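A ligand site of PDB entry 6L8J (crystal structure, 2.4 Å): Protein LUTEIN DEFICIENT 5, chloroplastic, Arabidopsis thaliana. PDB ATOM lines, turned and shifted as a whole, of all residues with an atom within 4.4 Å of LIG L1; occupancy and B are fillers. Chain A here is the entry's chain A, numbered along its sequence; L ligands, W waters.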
ATOM      1  N   LYS A  98      -2.826  34.753  36.246  1.00  0.00           N
ATOM      2  CA  LYS A  98      -1.928  34.659  35.094  1.00  0.00           C
ATOM      3  C   LYS A  98      -1.160  35.948  34.828  1.00  0.00           C
ATOM      4  O   LYS A  98      -0.215  35.920  34.035  1.00  0.00           O
ATOM      5  CB  LYS A  98      -2.711  34.234  33.851  1.00  0.00           C
ATOM      6  CG  LYS A  98      -3.117  32.753  33.830  1.00  0.00           C
ATOM      7  CD  LYS A  98      -1.930  31.869  34.209  1.00  0.00           C
ATOM      8  CE  LYS A  98      -2.237  30.395  34.047  1.00  0.00           C
ATOM      9  NZ  LYS A  98      -2.259  29.994  32.623  1.00  0.00           N
ATOM     10  N   LEU A 101       0.730  37.330  31.492  1.00  0.00           N
ATOM     11  CA  LEU A 101       0.336  36.385  30.458  1.00  0.00           C
ATOM     12  C   LEU A 101      -0.949  36.803  29.747  1.00  0.00           C
ATOM     13  O   LEU A 101      -1.053  36.706  28.526  1.00  0.00           O
ATOM     14  CB  LEU A 101       0.170  34.988  31.065  1.00  0.00           C
ATOM     15  CG  LEU A 101       0.073  33.832  30.082  1.00  0.00           C
ATOM     16  CD1 LEU A 101       1.392  33.707  29.354  1.00  0.00           C
ATOM     17  CD2 LEU A 101      -0.251  32.550  30.817  1.00  0.00           C
ATOM     18  N   LEU A 113      -8.727  29.431  27.899  1.00  0.00           N
ATOM     19  CA  LEU A 113      -8.294  28.877  29.181  1.00  0.00           C
ATOM     20  C   LEU A 113      -6.984  29.489  29.661  1.00  0.00           C
ATOM     21  O   LEU A 113      -6.872  29.900  30.825  1.00  0.00           O
ATOM     22  CB  LEU A 113      -8.191  27.360  29.084  1.00  0.00           C
ATOM     23  CG  LEU A 113      -9.484  26.573  29.209  1.00  0.00           C
ATOM     24  CD1 LEU A 113      -9.208  25.080  29.130  1.00  0.00           C
ATOM     25  CD2 LEU A 113     -10.197  26.914  30.501  1.00  0.00           C
ATOM     26  N   ILE A 114      -5.988  29.560  28.794  1.00  0.00           N
ATOM     27  CA  ILE A 114      -4.626  29.950  29.184  1.00  0.00           C
ATOM     28  C   ILE A 114      -4.605  31.292  29.915  1.00  0.00           C
ATOM     29  O   ILE A 114      -4.093  31.360  31.035  1.00  0.00           O
ATOM     30  CB  ILE A 114      -3.661  29.958  27.986  1.00  0.00           C
ATOM     31  CG1 ILE A 114      -3.368  28.524  27.536  1.00  0.00           C
ATOM     32  CG2 ILE A 114      -2.364  30.660  28.348  1.00  0.00           C
ATOM     33  CD1 ILE A 114      -2.544  28.424  26.277  1.00  0.00           C
ATOM     34  N   TRP A 121     -12.665  30.765  34.199  1.00  0.00           N
ATOM     35  CA  TRP A 121     -11.697  29.698  33.953  1.00  0.00           C
ATOM     36  C   TRP A 121     -12.227  28.359  34.454  1.00  0.00           C
ATOM     37  O   TRP A 121     -12.129  27.344  33.766  1.00  0.00           O
ATOM     38  CB  TRP A 121     -10.339  29.997  34.607  1.00  0.00           C
ATOM     39  CG  TRP A 121      -9.539  28.739  34.706  1.00  0.00           C
ATOM     40  CD1 TRP A 121      -8.827  28.133  33.714  1.00  0.00           C
ATOM     41  CD2 TRP A 121      -9.422  27.877  35.859  1.00  0.00           C
ATOM     42  NE1 TRP A 121      -8.260  26.969  34.172  1.00  0.00           N
ATOM     43  CE2 TRP A 121      -8.619  26.790  35.480  1.00  0.00           C
ATOM     44  CE3 TRP A 121      -9.916  27.936  37.165  1.00  0.00           C
ATOM     45  CZ2 TRP A 121      -8.281  25.763  36.365  1.00  0.00           C
ATOM     46  CZ3 TRP A 121      -9.593  26.915  38.036  1.00  0.00           C
ATOM     47  CH2 TRP A 121      -8.781  25.847  37.635  1.00  0.00           C
ATOM     48  N   ARG A 125     -12.797  25.222  31.998  1.00  0.00           N
ATOM     49  CA  ARG A 125     -11.955  24.049  32.204  1.00  0.00           C
ATOM     50  C   ARG A 125     -12.807  22.807  32.402  1.00  0.00           C
ATOM     51  O   ARG A 125     -12.510  21.754  31.832  1.00  0.00           O
ATOM     52  CB  ARG A 125     -11.032  24.268  33.409  1.00  0.00           C
ATOM     53  CG  ARG A 125     -10.290  23.012  33.846  1.00  0.00           C
ATOM     54  CD  ARG A 125      -8.846  23.043  33.404  1.00  0.00           C
ATOM     55  NE  ARG A 125      -8.094  21.900  33.920  1.00  0.00           N
ATOM     56  CZ  ARG A 125      -6.794  21.722  33.723  1.00  0.00           C
ATOM     57  NH1 ARG A 125      -6.104  22.613  33.026  1.00  0.00           N
ATOM     58  NH2 ARG A 125      -6.184  20.653  34.223  1.00  0.00           N
ATOM     59  N   ILE A 179      -3.360  20.126  14.429  1.00  0.00           N
ATOM     60  CA  ILE A 179      -4.186  20.759  15.449  1.00  0.00           C
ATOM     61  C   ILE A 179      -5.480  21.293  14.839  1.00  0.00           C
ATOM     62  O   ILE A 179      -6.531  21.283  15.499  1.00  0.00           O
ATOM     63  CB  ILE A 179      -3.397  21.865  16.185  1.00  0.00           C
ATOM     64  CG1 ILE A 179      -4.105  22.249  17.490  1.00  0.00           C
ATOM     65  CG2 ILE A 179      -3.172  23.087  15.300  1.00  0.00           C
ATOM     66  CD1 ILE A 179      -4.186  21.134  18.507  1.00  0.00           C
ATOM     67  N   MET A 298      -6.886  26.823  22.027  1.00  0.00           N
ATOM     68  CA  MET A 298      -6.317  25.501  21.815  1.00  0.00           C
ATOM     69  C   MET A 298      -5.565  25.412  20.488  1.00  0.00           C
ATOM     70  O   MET A 298      -4.568  24.691  20.391  1.00  0.00           O
ATOM     71  CB  MET A 298      -7.412  24.441  21.893  1.00  0.00           C
ATOM     72  CG  MET A 298      -7.913  24.211  23.307  1.00  0.00           C
ATOM     73  SD  MET A 298      -9.143  22.915  23.399  1.00  0.00           S
ATOM     74  CE  MET A 298     -10.607  23.808  22.863  1.00  0.00           C
ATOM     75  N   ALA A 301      -2.248  27.034  21.369  1.00  0.00           N
ATOM     76  CA  ALA A 301      -1.494  26.213  22.310  1.00  0.00           C
ATOM     77  C   ALA A 301      -0.932  24.965  21.636  1.00  0.00           C
ATOM     78  O   ALA A 301       0.255  24.656  21.772  1.00  0.00           O
ATOM     79  CB  ALA A 301      -2.394  25.839  23.488  1.00  0.00           C
ATOM     80  N   GLY A 302      -1.772  24.238  20.905  1.00  0.00           N
ATOM     81  CA  GLY A 302      -1.337  22.955  20.363  1.00  0.00           C
ATOM     82  C   GLY A 302      -0.434  23.050  19.166  1.00  0.00           C
ATOM     83  O   GLY A 302       0.118  22.017  18.756  1.00  0.00           O
ATOM     84  N   THR A 305       3.908  24.928  20.080  1.00  0.00           N
ATOM     85  CA  THR A 305       4.655  24.169  21.088  1.00  0.00           C
ATOM     86  C   THR A 305       5.247  22.892  20.499  1.00  0.00           C
ATOM     87  O   THR A 305       6.448  22.646  20.627  1.00  0.00           O
ATOM     88  CB  THR A 305       3.755  23.818  22.276  1.00  0.00           C
ATOM     89  OG1 THR A 305       2.572  23.166  21.795  1.00  0.00           O
ATOM     90  CG2 THR A 305       3.389  25.077  23.059  1.00  0.00           C
ATOM     91  N   SER A 306       4.424  22.073  19.860  1.00  0.00           N
ATOM     92  CA  SER A 306       4.942  20.830  19.309  1.00  0.00           C
ATOM     93  C   SER A 306       5.831  21.088  18.107  1.00  0.00           C
ATOM     94  O   SER A 306       6.790  20.329  17.886  1.00  0.00           O
ATOM     95  CB  SER A 306       3.792  19.882  18.945  1.00  0.00           C
ATOM     96  OG  SER A 306       3.272  19.269  20.116  1.00  0.00           O
ATOM     97  N   VAL A 309       9.000  21.451  19.717  1.00  0.00           N
ATOM     98  CA  VAL A 309       9.463  20.214  20.348  1.00  0.00           C
ATOM     99  C   VAL A 309      10.106  19.307  19.301  1.00  0.00           C
ATOM    100  O   VAL A 309      11.177  18.727  19.539  1.00  0.00           O
ATOM    101  CB  VAL A 309       8.298  19.517  21.065  1.00  0.00           C
ATOM    102  CG1 VAL A 309       8.711  18.123  21.506  1.00  0.00           C
ATOM    103  CG2 VAL A 309       7.867  20.339  22.273  1.00  0.00           C
ATOM    104  N   LEU A 359      11.993  17.990  25.767  1.00  0.00           N
ATOM    105  CA  LEU A 359      11.216  18.986  26.492  1.00  0.00           C
ATOM    106  C   LEU A 359      11.936  19.471  27.739  1.00  0.00           C
ATOM    107  O   LEU A 359      11.675  20.579  28.214  1.00  0.00           O
ATOM    108  CB  LEU A 359       9.841  18.428  26.855  1.00  0.00           C
ATOM    109  CG  LEU A 359       8.711  18.680  25.843  1.00  0.00           C
ATOM    110  CD1 LEU A 359       7.512  17.806  26.144  1.00  0.00           C
ATOM    111  CD2 LEU A 359       8.316  20.141  25.845  1.00  0.00           C
ATOM    112  N   GLN A 364       8.754  24.495  26.416  1.00  0.00           N
ATOM    113  CA  GLN A 364       7.855  25.341  25.625  1.00  0.00           C
ATOM    114  C   GLN A 364       6.629  25.653  26.483  1.00  0.00           C
ATOM    115  O   GLN A 364       5.717  24.816  26.579  1.00  0.00           O
ATOM    116  CB  GLN A 364       7.444  24.651  24.331  1.00  0.00           C
ATOM    117  CG  GLN A 364       8.584  24.030  23.553  1.00  0.00           C
ATOM    118  CD  GLN A 364       9.622  25.054  23.128  1.00  0.00           C
ATOM    119  OE1 GLN A 364       9.296  26.215  22.889  1.00  0.00           O
ATOM    120  NE2 GLN A 364      10.879  24.624  23.044  1.00  0.00           N
ATOM    121  N   PRO A 365       6.567  26.831  27.103  1.00  0.00           N
ATOM    122  CA  PRO A 365       7.533  27.937  27.092  1.00  0.00           C
ATOM    123  C   PRO A 365       8.656  27.750  28.118  1.00  0.00           C
ATOM    124  O   PRO A 365       8.478  27.010  29.085  1.00  0.00           O
ATOM    125  CB  PRO A 365       6.673  29.143  27.433  1.00  0.00           C
ATOM    126  CG  PRO A 365       5.652  28.583  28.375  1.00  0.00           C
ATOM    127  CD  PRO A 365       5.363  27.185  27.882  1.00  0.00           C
ATOM    128  N   LEU A 368       7.121  30.250  32.925  1.00  0.00           N
ATOM    129  CA  LEU A 368       5.718  30.368  33.293  1.00  0.00           C
ATOM    130  C   LEU A 368       5.506  31.670  34.061  1.00  0.00           C
ATOM    131  O   LEU A 368       6.385  32.113  34.806  1.00  0.00           O
ATOM    132  CB  LEU A 368       5.253  29.178  34.147  1.00  0.00           C
ATOM    133  CG  LEU A 368       5.298  27.809  33.451  1.00  0.00           C
ATOM    134  CD1 LEU A 368       4.730  26.735  34.361  1.00  0.00           C
ATOM    135  CD2 LEU A 368       4.531  27.846  32.143  1.00  0.00           C
ATOM    136  N   ARG A 370       3.123  34.307  36.419  1.00  0.00           N
ATOM    137  CA  ARG A 370       2.071  34.483  37.409  1.00  0.00           C
ATOM    138  C   ARG A 370       2.162  35.881  37.994  1.00  0.00           C
ATOM    139  O   ARG A 370       3.172  36.568  37.841  1.00  0.00           O
ATOM    140  CB  ARG A 370       2.168  33.451  38.551  1.00  0.00           C
ATOM    141  CG  ARG A 370       2.016  32.012  38.119  1.00  0.00           C
ATOM    142  CD  ARG A 370       0.581  31.698  37.763  1.00  0.00           C
ATOM    143  NE  ARG A 370       0.390  30.277  37.523  1.00  0.00           N
ATOM    144  CZ  ARG A 370       0.515  29.686  36.337  1.00  0.00           C
ATOM    145  NH1 ARG A 370       0.844  30.422  35.277  1.00  0.00           N
ATOM    146  NH2 ARG A 370       0.317  28.382  36.214  1.00  0.00           N
ATOM    147  N   PRO A 432       7.231  20.031  31.835  1.00  0.00           N
ATOM    148  CA  PRO A 432       6.965  20.227  30.407  1.00  0.00           C
ATOM    149  C   PRO A 432       5.565  20.729  30.137  1.00  0.00           C
ATOM    150  O   PRO A 432       5.360  21.482  29.173  1.00  0.00           O
ATOM    151  CB  PRO A 432       7.194  18.826  29.815  1.00  0.00           C
ATOM    152  CG  PRO A 432       6.959  17.902  30.940  1.00  0.00           C
ATOM    153  CD  PRO A 432       7.472  18.625  32.161  1.00  0.00           C
ATOM    154  N   PHE A 433       4.596  20.378  30.979  1.00  0.00           N
ATOM    155  CA  PHE A 433       3.209  20.765  30.775  1.00  0.00           C
ATOM    156  C   PHE A 433       2.653  21.560  31.953  1.00  0.00           C
ATOM    157  O   PHE A 433       1.435  21.709  32.092  1.00  0.00           O
ATOM    158  CB  PHE A 433       2.351  19.524  30.493  1.00  0.00           C
ATOM    159  CG  PHE A 433       2.780  18.779  29.274  1.00  0.00           C
ATOM    160  CD1 PHE A 433       2.377  19.192  28.008  1.00  0.00           C
ATOM    161  CD2 PHE A 433       3.618  17.683  29.375  1.00  0.00           C
ATOM    162  CE1 PHE A 433       2.789  18.528  26.888  1.00  0.00           C
ATOM    163  CE2 PHE A 433       4.025  17.011  28.250  1.00  0.00           C
ATOM    164  CZ  PHE A 433       3.619  17.426  27.008  1.00  0.00           C
ATOM    165  N   GLY A 434       3.526  22.070  32.807  1.00  0.00           N
ATOM    166  CA  GLY A 434       3.077  22.830  33.952  1.00  0.00           C
ATOM    167  C   GLY A 434       2.749  21.920  35.127  1.00  0.00           C
ATOM    168  O   GLY A 434       3.181  20.770  35.204  1.00  0.00           O
ATOM    169  N   PRO A 437      -3.497  23.200  39.193  1.00  0.00           N
ATOM    170  CA  PRO A 437      -4.805  23.259  38.516  1.00  0.00           C
ATOM    171  C   PRO A 437      -4.745  23.808  37.099  1.00  0.00           C
ATOM    172  O   PRO A 437      -5.644  23.518  36.305  1.00  0.00           O
ATOM    173  CB  PRO A 437      -5.651  24.167  39.419  1.00  0.00           C
ATOM    174  CG  PRO A 437      -4.813  24.413  40.664  1.00  0.00           C
ATOM    175  CD  PRO A 437      -3.393  24.194  40.283  1.00  0.00           C
ATOM    176  N   ARG A 438      -3.735  24.607  36.770  1.00  0.00           N
ATOM    177  CA  ARG A 438      -3.634  25.206  35.452  1.00  0.00           C
ATOM    178  C   ARG A 438      -2.802  24.358  34.489  1.00  0.00           C
ATOM    179  O   ARG A 438      -2.435  24.841  33.411  1.00  0.00           O
ATOM    180  CB  ARG A 438      -3.055  26.626  35.569  1.00  0.00           C
ATOM    181  CG  ARG A 438      -3.862  27.526  36.481  1.00  0.00           C
ATOM    182  CD  ARG A 438      -5.319  27.610  36.032  1.00  0.00           C
ATOM    183  NE  ARG A 438      -5.449  28.208  34.707  1.00  0.00           N
ATOM    184  CZ  ARG A 438      -5.710  29.489  34.485  1.00  0.00           C
ATOM    185  NH1 ARG A 438      -5.874  30.328  35.499  1.00  0.00           N
ATOM    186  NH2 ARG A 438      -5.795  29.943  33.232  1.00  0.00           N
ATOM    187  N   LYS A 439      -2.523  23.103  34.859  1.00  0.00           N
ATOM    188  CA  LYS A 439      -1.720  22.225  34.036  1.00  0.00           C
ATOM    189  C   LYS A 439      -2.330  22.052  32.650  1.00  0.00           C
ATOM    190  O   LYS A 439      -3.539  22.144  32.465  1.00  0.00           O
ATOM    191  CB  LYS A 439      -1.562  20.860  34.716  1.00  0.00           C
ATOM    192  CG  LYS A 439      -0.584  19.930  34.017  1.00  0.00           C
ATOM    193  CD  LYS A 439      -0.514  18.583  34.709  1.00  0.00           C
ATOM    194  CE  LYS A 439       0.454  17.653  34.001  1.00  0.00           C
ATOM    195  NZ  LYS A 439       0.281  16.251  34.480  1.00  0.00           N
ATOM    196  N   CYS A 440      -1.467  21.819  31.672  1.00  0.00           N
ATOM    197  CA  CYS A 440      -1.900  21.585  30.304  1.00  0.00           C
ATOM    198  C   CYS A 440      -2.926  20.460  30.235  1.00  0.00           C
ATOM    199  O   CYS A 440      -2.734  19.383  30.819  1.00  0.00           O
ATOM    200  CB  CYS A 440      -0.686  21.230  29.440  1.00  0.00           C
ATOM    201  SG  CYS A 440      -1.085  20.707  27.785  1.00  0.00           S
ATOM    202  N   ILE A 441      -4.027  20.715  29.520  1.00  0.00           N
ATOM    203  CA  ILE A 441      -5.019  19.680  29.269  1.00  0.00           C
ATOM    204  C   ILE A 441      -4.690  18.838  28.040  1.00  0.00           C
ATOM    205  O   ILE A 441      -5.351  17.822  27.802  1.00  0.00           O
ATOM    206  CB  ILE A 441      -6.424  20.273  29.065  1.00  0.00           C
ATOM    207  CG1 ILE A 441      -6.494  21.041  27.748  1.00  0.00           C
ATOM    208  CG2 ILE A 441      -6.798  21.168  30.235  1.00  0.00           C
ATOM    209  CD1 ILE A 441      -7.834  21.662  27.479  1.00  0.00           C
ATOM    210  N   GLY A 442      -3.702  19.256  27.248  1.00  0.00           N
ATOM    211  CA  GLY A 442      -3.363  18.524  26.054  1.00  0.00           C
ATOM    212  C   GLY A 442      -2.094  17.709  26.201  1.00  0.00           C
ATOM    213  O   GLY A 442      -1.463  17.361  25.201  1.00  0.00           O
ATOM    214  N   PHE A 445      -2.399  14.248  24.524  1.00  0.00           N
ATOM    215  CA  PHE A 445      -2.518  14.575  23.105  1.00  0.00           C
ATOM    216  C   PHE A 445      -1.142  14.834  22.494  1.00  0.00           C
ATOM    217  O   PHE A 445      -0.707  14.137  21.573  1.00  0.00           O
ATOM    218  CB  PHE A 445      -3.439  15.782  22.943  1.00  0.00           C
ATOM    219  CG  PHE A 445      -3.713  16.163  21.514  1.00  0.00           C
ATOM    220  CD1 PHE A 445      -2.778  16.879  20.775  1.00  0.00           C
ATOM    221  CD2 PHE A 445      -4.909  15.835  20.915  1.00  0.00           C
ATOM    222  CE1 PHE A 445      -3.025  17.241  19.466  1.00  0.00           C
ATOM    223  CE2 PHE A 445      -5.168  16.196  19.596  1.00  0.00           C
ATOM    224  CZ  PHE A 445      -4.229  16.899  18.876  1.00  0.00           C
ATOM    225  N   ALA A 446      -0.432  15.827  23.049  1.00  0.00           N
ATOM    226  CA  ALA A 446       0.829  16.283  22.459  1.00  0.00           C
ATOM    227  C   ALA A 446       1.950  15.274  22.684  1.00  0.00           C
ATOM    228  O   ALA A 446       2.826  15.121  21.816  1.00  0.00           O
ATOM    229  CB  ALA A 446       1.206  17.650  23.036  1.00  0.00           C
ATOM    230  N   ASN A 450       3.901  13.834  19.336  1.00  0.00           N
ATOM    231  CA  ASN A 450       5.330  13.974  19.084  1.00  0.00           C
ATOM    232  C   ASN A 450       6.020  12.615  18.972  1.00  0.00           C
ATOM    233  O   ASN A 450       6.919  12.437  18.142  1.00  0.00           O
ATOM    234  CB  ASN A 450       5.962  14.838  20.166  1.00  0.00           C
ATOM    235  CG  ASN A 450       5.514  16.284  20.068  1.00  0.00           C
ATOM    236  OD1 ASN A 450       5.614  16.891  19.005  1.00  0.00           O
ATOM    237  ND2 ASN A 450       4.993  16.829  21.158  1.00  0.00           N
HETATM  238  C1  LIG L   1      -1.678  25.011  29.283  1.00  0.00           C
HETATM  239  C2  LIG L   1       2.523  23.361  27.497  1.00  0.00           C
HETATM  240  C3  LIG L   1       0.191  21.303  23.767  1.00  0.00           C
HETATM  241  C4  LIG L   1      -3.968  23.192  25.388  1.00  0.00           C
HETATM  242  C5  LIG L   1      -0.333  24.711  29.169  1.00  0.00           C
HETATM  243  C6  LIG L   1       0.720  24.997  30.131  1.00  0.00           C
HETATM  244  C7  LIG L   1       1.871  24.541  29.628  1.00  0.00           C
HETATM  245  C8  LIG L   1       1.591  23.946  28.332  1.00  0.00           C
HETATM  246  C9  LIG L   1       3.265  24.619  30.285  1.00  0.00           C
HETATM  247  C10 LIG L   1       0.541  25.704  31.498  1.00  0.00           C
HETATM  248  C11 LIG L   1       0.675  27.218  31.310  1.00  0.00           C
HETATM  249  C12 LIG L   1       0.542  27.941  32.635  1.00  0.00           C
HETATM  250  O1  LIG L   1       0.521  27.283  33.708  1.00  0.00           O
HETATM  251  O2  LIG L   1       0.460  29.184  32.607  1.00  0.00           O
HETATM  252  C13 LIG L   1       2.269  22.651  26.347  1.00  0.00           C
HETATM  253  C14 LIG L   1       3.242  21.925  25.538  1.00  0.00           C
HETATM  254  C15 LIG L   1       2.594  21.364  24.500  1.00  0.00           C
HETATM  255  C16 LIG L   1       1.195  21.710  24.629  1.00  0.00           C
HETATM  256  C17 LIG L   1       4.760  21.864  25.864  1.00  0.00           C
HETATM  257  C18 LIG L   1       3.134  20.486  23.344  1.00  0.00           C
HETATM  258  C19 LIG L   1       4.349  19.927  23.304  1.00  0.00           C
HETATM  259  C20 LIG L   1      -1.148  21.563  23.918  1.00  0.00           C
HETATM  260  C21 LIG L   1      -2.219  20.975  23.151  1.00  0.00           C
HETATM  261  C22 LIG L   1      -3.384  21.468  23.583  1.00  0.00           C
HETATM  262  C23 LIG L   1      -3.092  22.427  24.657  1.00  0.00           C
HETATM  263  C24 LIG L   1      -2.052  19.934  22.028  1.00  0.00           C
HETATM  264  C25 LIG L   1      -4.750  21.052  22.976  1.00  0.00           C
HETATM  265  C26 LIG L   1      -5.911  21.319  23.586  1.00  0.00           C
HETATM  266  C27 LIG L   1      -3.718  23.877  26.564  1.00  0.00           C
HETATM  267  C28 LIG L   1      -4.674  24.635  27.343  1.00  0.00           C
HETATM  268  C29 LIG L   1      -4.050  25.136  28.420  1.00  0.00           C
HETATM  269  C30 LIG L   1      -2.661  24.705  28.360  1.00  0.00           C
HETATM  270  C31 LIG L   1      -6.163  24.827  26.988  1.00  0.00           C
HETATM  271  C32 LIG L   1      -4.679  26.006  29.538  1.00  0.00           C
HETATM  272  C33 LIG L   1      -5.192  25.104  30.653  1.00  0.00           C
HETATM  273  C34 LIG L   1      -5.727  25.924  31.807  1.00  0.00           C
HETATM  274  O3  LIG L   1      -6.665  25.439  32.503  1.00  0.00           O
HETATM  275  O4  LIG L   1      -5.226  27.051  32.036  1.00  0.00           O
HETATM  276  N1  LIG L   1       0.244  24.066  28.087  1.00  0.00           N
HETATM  277  N2  LIG L   1       1.028  22.488  25.756  1.00  0.00           N
HETATM  278  N3  LIG L   1      -1.722  22.442  24.827  1.00  0.00           N
HETATM  279  N4  LIG L   1      -2.504  23.940  27.223  1.00  0.00           N
HETATM  280 FE1  LIG L   1      -0.811  23.019  26.629  1.00  0.00          FE
HETATM  281  C1  LG2 L   2       1.710  28.833  24.734  1.00  0.00           C
HETATM  282  C2  LG2 L   2       0.966  27.502  24.850  1.00  0.00           C
HETATM  283  C3  LG2 L   2       1.387  26.656  26.034  1.00  0.00           C
HETATM  284  C4  LG2 L   2       1.318  27.399  27.361  1.00  0.00           C
HETATM  285  C5  LG2 L   2       1.421  28.898  27.241  1.00  0.00           C
HETATM  286  C6  LG2 L   2       1.815  29.504  26.105  1.00  0.00           C
HETATM  287  C7  LG2 L   2       2.295  30.878  26.070  1.00  0.00           C
HETATM  288  C8  LG2 L   2       3.402  31.285  26.647  1.00  0.00           C
HETATM  289  C9  LG2 L   2       3.986  32.610  26.658  1.00  0.00           C
HETATM  290  C10 LG2 L   2       5.263  32.739  27.041  1.00  0.00           C
HETATM  291  C11 LG2 L   2       6.074  33.921  27.125  1.00  0.00           C
HETATM  292  C12 LG2 L   2       7.266  33.871  27.696  1.00  0.00           C
HETATM  293  C13 LG2 L   2       8.239  34.927  27.860  1.00  0.00           C
HETATM  294  C14 LG2 L   2       9.555  34.607  27.748  1.00  0.00           C
HETATM  295  C15 LG2 L   2      10.691  35.478  27.877  1.00  0.00           C
HETATM  296  O1  LG2 L   2      11.838  35.098  27.755  1.00  0.00           O
HETATM  297  C16 LG2 L   2       3.105  28.584  24.171  1.00  0.00           C
HETATM  298  C17 LG2 L   2       0.957  29.743  23.757  1.00  0.00           C
HETATM  299  C18 LG2 L   2       1.270  29.608  28.566  1.00  0.00           C
HETATM  300  C19 LG2 L   2       3.119  33.763  26.227  1.00  0.00           C
HETATM  301  C20 LG2 L   2       7.739  36.309  28.141  1.00  0.00           C
HETATM  302  O   HOH W   1       0.823  24.802  35.081  1.00  0.00           O
HETATM  303  O   HOH W   2       0.745  19.812  20.229  1.00  0.00           O
HETATM  304  O   HOH W   3      -2.541  27.331  31.958  1.00  0.00           O
HETATM  305  O   HOH W   4       6.735  24.700  30.075  1.00  0.00           O
HETATM  306  O   HOH W   5       2.510  31.068  31.890  1.00  0.00           O
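The side-chain sulfur of Cys 440 is bound to an iron atom (FE1) of LIG L1, 2.6 Å away.
The side-chain amino group (NZ) of Lys 98 is in salt-bridge range of an oxygen (O2) of LIG L1, at 2.8 Å.
NE of Arg 438 is in salt-bridge range of O4 of LIG L1, at 2.9 Å.
The guanidinium group (NH1) of Arg 125 lies within salt-bridge range of an oxygen (O3) of LIG L1 (2.9 Å).
An oxygen (O3) of LIG L1 lies within hydrogen-bond range of the indole nitrogen (NE1) of Trp 121 (2.8 Å).
An oxygen (O1) of LIG L1 lies within salt-bridge range of the guanidinium group of Arg 370.
NH1 of Arg 125 is in hydrogen-bond range of O of Lys 439, at 2.7 Å.
O of Pro 437 lies close to NH1 of Arg 125.
The side-chain hydroxyl of Thr 305 sits at hydrogen-bond distance from the backbone carbonyl oxygen of Ala 301 (2.8 Å).
The backbone carbonyl oxygen (O) of Ala 446 lies within hydrogen-bond range of the side-chain amide nitrogen (ND2) of Asn 450, 2.8 Å away.
The guanidinium group (NH2) of Arg 438 is in hydrogen-bond range of the backbone carbonyl oxygen (O) of Ile 114, at 3.1 Å.
The side-chain hydroxyl (OG) of Ser 306 is in hydrogen-bond range of the side-chain amide nitrogen (ND2) of Asn 450.
The backbone carbonyl oxygen of Leu 113 lies within hydrogen-bond range of the guanidinium group of Arg 438, at 2.6 Å.
The backbone NH of Cys 440 is in hydrogen-bond range of the backbone carbonyl oxygen of Phe 433 (2.9 Å).
Merely in contact with LIG L1: Thr 305, Gln 364, Phe 445, Pro 432, Ser 306, Ala 446, Ile 114, Leu 113, Gly 302, Met 298, Phe 433, Gly 434, Ile 441, Ala 301, Val 309, Asn 450, Gly 442, Lys 439, Leu 101, Leu 368 and Leu 359.
27 residues have an atom within 4 Å of LIG L1: Lys 98, Leu 101, Leu 113, Ile 114, Trp 121, Arg 125, Met 298, Ala 301, Gly 302, Thr 305, Ser 306, Val 309, Leu 359, Gln 364, Leu 368, Arg 370, Pro 432, Phe 433, Gly 434, Arg 438, Lys 439, Cys 440, Ile 441, Gly 442, Phe 445, Ala 446 and Asn 450.
Water W3 lies within hydrogen-bond range of an oxygen (O4) of LIG L1 (2.7 Å), the side-chain amino group (NZ) of Lys 98 (2.8 Å) and the backbone carbonyl oxygen (O) of Arg 438 (2.9 Å).
Water W2 bridges OG of Ser 306 and O of Gly 302.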
